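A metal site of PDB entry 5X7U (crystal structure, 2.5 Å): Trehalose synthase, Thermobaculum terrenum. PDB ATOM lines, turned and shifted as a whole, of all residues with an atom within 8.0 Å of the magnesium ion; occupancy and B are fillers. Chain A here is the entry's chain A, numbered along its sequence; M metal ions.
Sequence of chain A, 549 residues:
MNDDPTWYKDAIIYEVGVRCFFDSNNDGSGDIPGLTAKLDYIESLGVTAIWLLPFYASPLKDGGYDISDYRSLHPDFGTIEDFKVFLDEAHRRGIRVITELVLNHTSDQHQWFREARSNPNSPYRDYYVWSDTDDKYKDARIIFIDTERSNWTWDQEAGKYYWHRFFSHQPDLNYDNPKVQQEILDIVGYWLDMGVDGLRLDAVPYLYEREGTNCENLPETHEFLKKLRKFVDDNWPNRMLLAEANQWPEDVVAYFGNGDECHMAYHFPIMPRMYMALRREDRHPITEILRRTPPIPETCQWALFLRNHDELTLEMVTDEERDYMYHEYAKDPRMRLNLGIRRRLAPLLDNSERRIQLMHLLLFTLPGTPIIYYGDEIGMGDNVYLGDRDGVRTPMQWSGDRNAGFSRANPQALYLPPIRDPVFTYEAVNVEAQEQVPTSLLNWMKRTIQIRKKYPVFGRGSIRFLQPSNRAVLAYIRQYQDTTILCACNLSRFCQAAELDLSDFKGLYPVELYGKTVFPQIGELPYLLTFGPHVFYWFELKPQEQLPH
The side-chain hydroxyl (OG) of Ser 407 sits at hydrogen-bond distance from the side-chain carboxylate (OD2) of Asp 23 (2.8 Å). The backbone carbonyl oxygen of Val 18 lies within hydrogen-bond range of the backbone NH of Asp 31. The side-chain carboxylate of Asp 31 sits at hydrogen-bond distance from the side-chain hydroxyl of Ser 24 (2.4 Å). OD2 of Asp 23 lies close to N of Asn 26 (3.2 Å). The backbone carbonyl oxygen of Phe 22 sits at hydrogen-bond distance from the backbone NH of Asp 31, at 3.1 Å. The backbone NH (N) of Gly 28 lies within hydrogen-bond range of the side-chain carboxylate (OD2) of Asp 23, at 2.8 Å. The side-chain carboxylate (OD1) of Asp 31 lies within hydrogen-bond range of the backbone NH (N) of Gly 34 (2.8 Å). OG of Ser 29 is in hydrogen-bond range of NE of Arg 19 (3.3 Å).
OD1 of Asp 23 is bound to the magnesium ion, 2.2 Å away. The backbone carbonyl oxygen (O) of Ser 29 is bound to the magnesium ion. OD2 of Asp 31 is bound to the magnesium ion. OD1 of Asn 25 binds the magnesium ion (2.3 Å). The magnesium ion is bound by OD1 of Asp 27, 2.4 Å away. The magnesium ion has five donor atoms within binding distance.
Five residues have an atom within 4 Å of the magnesium ion: Asp 23, Asn 25, Asp 27, Ser 29 and Asp 31.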
ATOM      1  N   VAL A  18     -23.610   3.097  10.355  1.00  0.00           N
ATOM      2  CA  VAL A  18     -23.680   3.522   8.955  1.00  0.00           C
ATOM      3  C   VAL A  18     -24.298   2.436   8.094  1.00  0.00           C
ATOM      4  O   VAL A  18     -25.134   2.711   7.217  1.00  0.00           O
ATOM      5  CB  VAL A  18     -22.279   3.905   8.448  1.00  0.00           C
ATOM      6  CG1 VAL A  18     -22.355   4.315   6.983  1.00  0.00           C
ATOM      7  CG2 VAL A  18     -21.684   5.012   9.303  1.00  0.00           C
ATOM      8  N   ARG A  19     -23.907   1.188   8.335  1.00  0.00           N
ATOM      9  CA  ARG A  19     -24.405   0.079   7.527  1.00  0.00           C
ATOM     10  C   ARG A  19     -25.890  -0.138   7.706  1.00  0.00           C
ATOM     11  O   ARG A  19     -26.530  -0.714   6.824  1.00  0.00           O
ATOM     12  CB  ARG A  19     -23.606  -1.186   7.861  1.00  0.00           C
ATOM     13  CG  ARG A  19     -24.152  -2.458   7.305  1.00  0.00           C
ATOM     14  CD  ARG A  19     -23.089  -3.525   7.217  1.00  0.00           C
ATOM     15  NE  ARG A  19     -22.401  -3.334   5.952  1.00  0.00           N
ATOM     16  CZ  ARG A  19     -22.012  -4.323   5.159  1.00  0.00           C
ATOM     17  NH1 ARG A  19     -22.224  -5.597   5.507  1.00  0.00           N
ATOM     18  NH2 ARG A  19     -21.425  -4.023   4.014  1.00  0.00           N
ATOM     19  N   PHE A  22     -29.197   4.024   5.954  1.00  0.00           N
ATOM     20  CA  PHE A  22     -29.817   4.245   4.648  1.00  0.00           C
ATOM     21  C   PHE A  22     -28.840   3.908   3.532  1.00  0.00           C
ATOM     22  O   PHE A  22     -27.693   4.376   3.537  1.00  0.00           O
ATOM     23  CB  PHE A  22     -30.296   5.689   4.503  1.00  0.00           C
ATOM     24  CG  PHE A  22     -31.094   5.939   3.244  1.00  0.00           C
ATOM     25  CD1 PHE A  22     -32.306   5.285   3.037  1.00  0.00           C
ATOM     26  CD2 PHE A  22     -30.649   6.839   2.288  1.00  0.00           C
ATOM     27  CE1 PHE A  22     -33.061   5.511   1.884  1.00  0.00           C
ATOM     28  CE2 PHE A  22     -31.393   7.079   1.122  1.00  0.00           C
ATOM     29  CZ  PHE A  22     -32.600   6.418   0.926  1.00  0.00           C
ATOM     30  N   ASP A  23     -29.302   3.068   2.602  1.00  0.00           N
ATOM     31  CA  ASP A  23     -28.526   2.633   1.450  1.00  0.00           C
ATOM     32  C   ASP A  23     -28.825   3.581   0.288  1.00  0.00           C
ATOM     33  O   ASP A  23     -29.927   3.573  -0.263  1.00  0.00           O
ATOM     34  CB  ASP A  23     -28.880   1.194   1.078  1.00  0.00           C
ATOM     35  CG  ASP A  23     -28.091   0.674  -0.117  1.00  0.00           C
ATOM     36  OD1 ASP A  23     -27.006   1.223  -0.442  1.00  0.00           O
ATOM     37  OD2 ASP A  23     -28.559  -0.321  -0.714  1.00  0.00           O
ATOM     38  N   SER A  24     -27.842   4.421  -0.072  1.00  0.00           N
ATOM     39  CA  SER A  24     -28.057   5.434  -1.103  1.00  0.00           C
ATOM     40  C   SER A  24     -27.821   4.938  -2.520  1.00  0.00           C
ATOM     41  O   SER A  24     -28.413   5.469  -3.443  1.00  0.00           O
ATOM     42  CB  SER A  24     -27.156   6.644  -0.863  1.00  0.00           C
ATOM     43  OG  SER A  24     -25.783   6.291  -0.977  1.00  0.00           O
ATOM     44  N   ASN A  25     -26.956   3.937  -2.710  1.00  0.00           N
ATOM     45  CA  ASN A  25     -26.687   3.381  -4.035  1.00  0.00           C
ATOM     46  C   ASN A  25     -27.353   2.026  -4.272  1.00  0.00           C
ATOM     47  O   ASN A  25     -27.095   1.419  -5.317  1.00  0.00           O
ATOM     48  CB  ASN A  25     -25.186   3.222  -4.237  1.00  0.00           C
ATOM     49  CG  ASN A  25     -24.614   2.215  -3.292  1.00  0.00           C
ATOM     50  OD1 ASN A  25     -25.193   1.946  -2.227  1.00  0.00           O
ATOM     51  ND2 ASN A  25     -23.477   1.648  -3.645  1.00  0.00           N
ATOM     52  N   ASN A  26     -28.123   1.504  -3.330  1.00  0.00           N
ATOM     53  CA  ASN A  26     -28.955   0.328  -3.561  1.00  0.00           C
ATOM     54  C   ASN A  26     -28.130  -0.933  -3.825  1.00  0.00           C
ATOM     55  O   ASN A  26     -28.497  -1.755  -4.679  1.00  0.00           O
ATOM     56  CB  ASN A  26     -29.946   0.563  -4.689  1.00  0.00           C
ATOM     57  CG  ASN A  26     -30.829   1.781  -4.444  1.00  0.00           C
ATOM     58  OD1 ASN A  26     -31.396   1.950  -3.359  1.00  0.00           O
ATOM     59  ND2 ASN A  26     -30.937   2.639  -5.445  1.00  0.00           N
ATOM     60  N   ASP A  27     -27.033  -1.103  -3.098  1.00  0.00           N
ATOM     61  CA  ASP A  27     -26.262  -2.333  -3.115  1.00  0.00           C
ATOM     62  C   ASP A  27     -26.578  -3.251  -1.938  1.00  0.00           C
ATOM     63  O   ASP A  27     -25.940  -4.295  -1.780  1.00  0.00           O
ATOM     64  CB  ASP A  27     -24.760  -2.027  -3.143  1.00  0.00           C
ATOM     65  CG  ASP A  27     -24.296  -1.209  -1.930  1.00  0.00           C
ATOM     66  OD1 ASP A  27     -25.141  -0.823  -1.115  1.00  0.00           O
ATOM     67  OD2 ASP A  27     -23.093  -0.933  -1.805  1.00  0.00           O
ATOM     68  N   GLY A  28     -27.543  -2.878  -1.094  1.00  0.00           N
ATOM     69  CA  GLY A  28     -27.920  -3.682   0.040  1.00  0.00           C
ATOM     70  C   GLY A  28     -27.304  -3.267   1.360  1.00  0.00           C
ATOM     71  O   GLY A  28     -27.659  -3.835   2.401  1.00  0.00           O
ATOM     72  N   SER A  29     -26.408  -2.283   1.346  1.00  0.00           N
ATOM     73  CA  SER A  29     -25.736  -1.859   2.557  1.00  0.00           C
ATOM     74  C   SER A  29     -25.882  -0.364   2.755  1.00  0.00           C
ATOM     75  O   SER A  29     -25.754   0.419   1.803  1.00  0.00           O
ATOM     76  CB  SER A  29     -24.273  -2.235   2.515  1.00  0.00           C
ATOM     77  OG  SER A  29     -23.568  -1.498   3.477  1.00  0.00           O
ATOM     78  N   GLY A  30     -26.146   0.049   3.994  1.00  0.00           N
ATOM     79  CA  GLY A  30     -26.157   1.463   4.292  1.00  0.00           C
ATOM     80  C   GLY A  30     -24.799   2.101   4.082  1.00  0.00           C
ATOM     81  O   GLY A  30     -23.765   1.438   4.146  1.00  0.00           O
ATOM     82  N   ASP A  31     -24.796   3.409   3.813  1.00  0.00           N
ATOM     83  CA  ASP A  31     -23.542   4.080   3.515  1.00  0.00           C
ATOM     84  C   ASP A  31     -23.564   5.518   4.000  1.00  0.00           C
ATOM     85  O   ASP A  31     -24.606   6.076   4.363  1.00  0.00           O
ATOM     86  CB  ASP A  31     -23.250   4.041   2.019  1.00  0.00           C
ATOM     87  CG  ASP A  31     -24.449   4.419   1.188  1.00  0.00           C
ATOM     88  OD1 ASP A  31     -24.760   5.634   1.128  1.00  0.00           O
ATOM     89  OD2 ASP A  31     -25.074   3.496   0.603  1.00  0.00           O
ATOM     90  N   ILE A  32     -22.373   6.127   3.987  1.00  0.00           N
ATOM     91  CA  ILE A  32     -22.233   7.502   4.488  1.00  0.00           C
ATOM     92  C   ILE A  32     -23.029   8.510   3.685  1.00  0.00           C
ATOM     93  O   ILE A  32     -23.718   9.346   4.296  1.00  0.00           O
ATOM     94  CB  ILE A  32     -20.749   7.862   4.605  1.00  0.00           C
ATOM     95  CG1 ILE A  32     -20.114   7.020   5.699  1.00  0.00           C
ATOM     96  CG2 ILE A  32     -20.566   9.340   4.891  1.00  0.00           C
ATOM     97  CD1 ILE A  32     -18.757   7.468   6.080  1.00  0.00           C
ATOM     98  N   PRO A  33     -23.020   8.513   2.350  1.00  0.00           N
ATOM     99  CA  PRO A  33     -23.918   9.443   1.636  1.00  0.00           C
ATOM    100  C   PRO A  33     -25.381   9.227   1.977  1.00  0.00           C
ATOM    101  O   PRO A  33     -26.155  10.185   2.026  1.00  0.00           O
ATOM    102  CB  PRO A  33     -23.623   9.153   0.148  1.00  0.00           C
ATOM    103  CG  PRO A  33     -22.249   8.519   0.136  1.00  0.00           C
ATOM    104  CD  PRO A  33     -22.160   7.746   1.418  1.00  0.00           C
ATOM    105  N   GLY A  34     -25.786   7.967   2.210  1.00  0.00           N
ATOM    106  CA  GLY A  34     -27.157   7.729   2.648  1.00  0.00           C
ATOM    107  C   GLY A  34     -27.417   8.318   4.022  1.00  0.00           C
ATOM    108  O   GLY A  34     -28.468   8.933   4.260  1.00  0.00           O
ATOM    109  N   PRO A  75     -15.093  -0.220   2.179  1.00  0.00           N
ATOM    110  CA  PRO A  75     -15.581   0.171   0.839  1.00  0.00           C
ATOM    111  C   PRO A  75     -17.092   0.310   0.729  1.00  0.00           C
ATOM    112  O   PRO A  75     -17.561   1.131  -0.058  1.00  0.00           O
ATOM    113  CB  PRO A  75     -15.066  -0.964  -0.062  1.00  0.00           C
ATOM    114  CG  PRO A  75     -13.988  -1.619   0.708  1.00  0.00           C
ATOM    115  CD  PRO A  75     -14.299  -1.461   2.148  1.00  0.00           C
ATOM    116  N   ASP A  76     -17.869  -0.473   1.474  1.00  0.00           N
ATOM    117  CA  ASP A  76     -19.324  -0.345   1.355  1.00  0.00           C
ATOM    118  C   ASP A  76     -19.860   0.965   1.892  1.00  0.00           C
ATOM    119  O   ASP A  76     -21.008   1.324   1.590  1.00  0.00           O
ATOM    120  CB  ASP A  76     -20.019  -1.496   2.066  1.00  0.00           C
ATOM    121  CG  ASP A  76     -19.696  -2.820   1.464  1.00  0.00           C
ATOM    122  OD1 ASP A  76     -20.171  -3.853   1.996  1.00  0.00           O
ATOM    123  OD2 ASP A  76     -18.951  -2.835   0.455  1.00  0.00           O
ATOM    124  N   PHE A  77     -19.081   1.691   2.703  1.00  0.00           N
ATOM    125  CA  PHE A  77     -19.583   2.892   3.364  1.00  0.00           C
ATOM    126  C   PHE A  77     -19.177   4.185   2.667  1.00  0.00           C
ATOM    127  O   PHE A  77     -19.735   5.234   2.989  1.00  0.00           O
ATOM    128  CB  PHE A  77     -19.122   2.932   4.819  1.00  0.00           C
ATOM    129  CG  PHE A  77     -19.504   1.710   5.596  1.00  0.00           C
ATOM    130  CD1 PHE A  77     -20.601   0.932   5.212  1.00  0.00           C
ATOM    131  CD2 PHE A  77     -18.781   1.336   6.723  1.00  0.00           C
ATOM    132  CE1 PHE A  77     -20.959  -0.204   5.933  1.00  0.00           C
ATOM    133  CE2 PHE A  77     -19.133   0.202   7.459  1.00  0.00           C
ATOM    134  CZ  PHE A  77     -20.210  -0.566   7.066  1.00  0.00           C
ATOM    135  N   GLY A  78     -18.255   4.127   1.722  1.00  0.00           N
ATOM    136  CA  GLY A  78     -17.852   5.316   1.004  1.00  0.00           C
ATOM    137  C   GLY A  78     -16.378   5.644   1.175  1.00  0.00           C
ATOM    138  O   GLY A  78     -15.573   4.790   1.542  1.00  0.00           O
ATOM    139  N   PHE A 406     -35.436   1.206   3.262  1.00  0.00           N
ATOM    140  CA  PHE A 406     -34.014   1.345   3.537  1.00  0.00           C
ATOM    141  C   PHE A 406     -33.173   1.225   2.268  1.00  0.00           C
ATOM    142  O   PHE A 406     -32.041   1.727   2.229  1.00  0.00           O
ATOM    143  CB  PHE A 406     -33.602   0.286   4.573  1.00  0.00           C
ATOM    144  CG  PHE A 406     -32.145  -0.086   4.552  1.00  0.00           C
ATOM    145  CD1 PHE A 406     -31.195   0.675   5.250  1.00  0.00           C
ATOM    146  CD2 PHE A 406     -31.703  -1.221   3.880  1.00  0.00           C
ATOM    147  CE1 PHE A 406     -29.856   0.315   5.254  1.00  0.00           C
ATOM    148  CE2 PHE A 406     -30.360  -1.579   3.876  1.00  0.00           C
ATOM    149  CZ  PHE A 406     -29.434  -0.822   4.573  1.00  0.00           C
ATOM    150  N   SER A 407     -33.710   0.605   1.239  1.00  0.00           N
ATOM    151  CA  SER A 407     -32.936   0.274   0.058  1.00  0.00           C
ATOM    152  C   SER A 407     -33.896  -0.075  -1.066  1.00  0.00           C
ATOM    153  O   SER A 407     -35.042  -0.468  -0.828  1.00  0.00           O
ATOM    154  CB  SER A 407     -31.977  -0.886   0.330  1.00  0.00           C
ATOM    155  OG  SER A 407     -31.200  -1.202  -0.810  1.00  0.00           O
HETATM  156 MG    MG M   1     -24.821   1.312  -0.046  1.00  0.00          MG
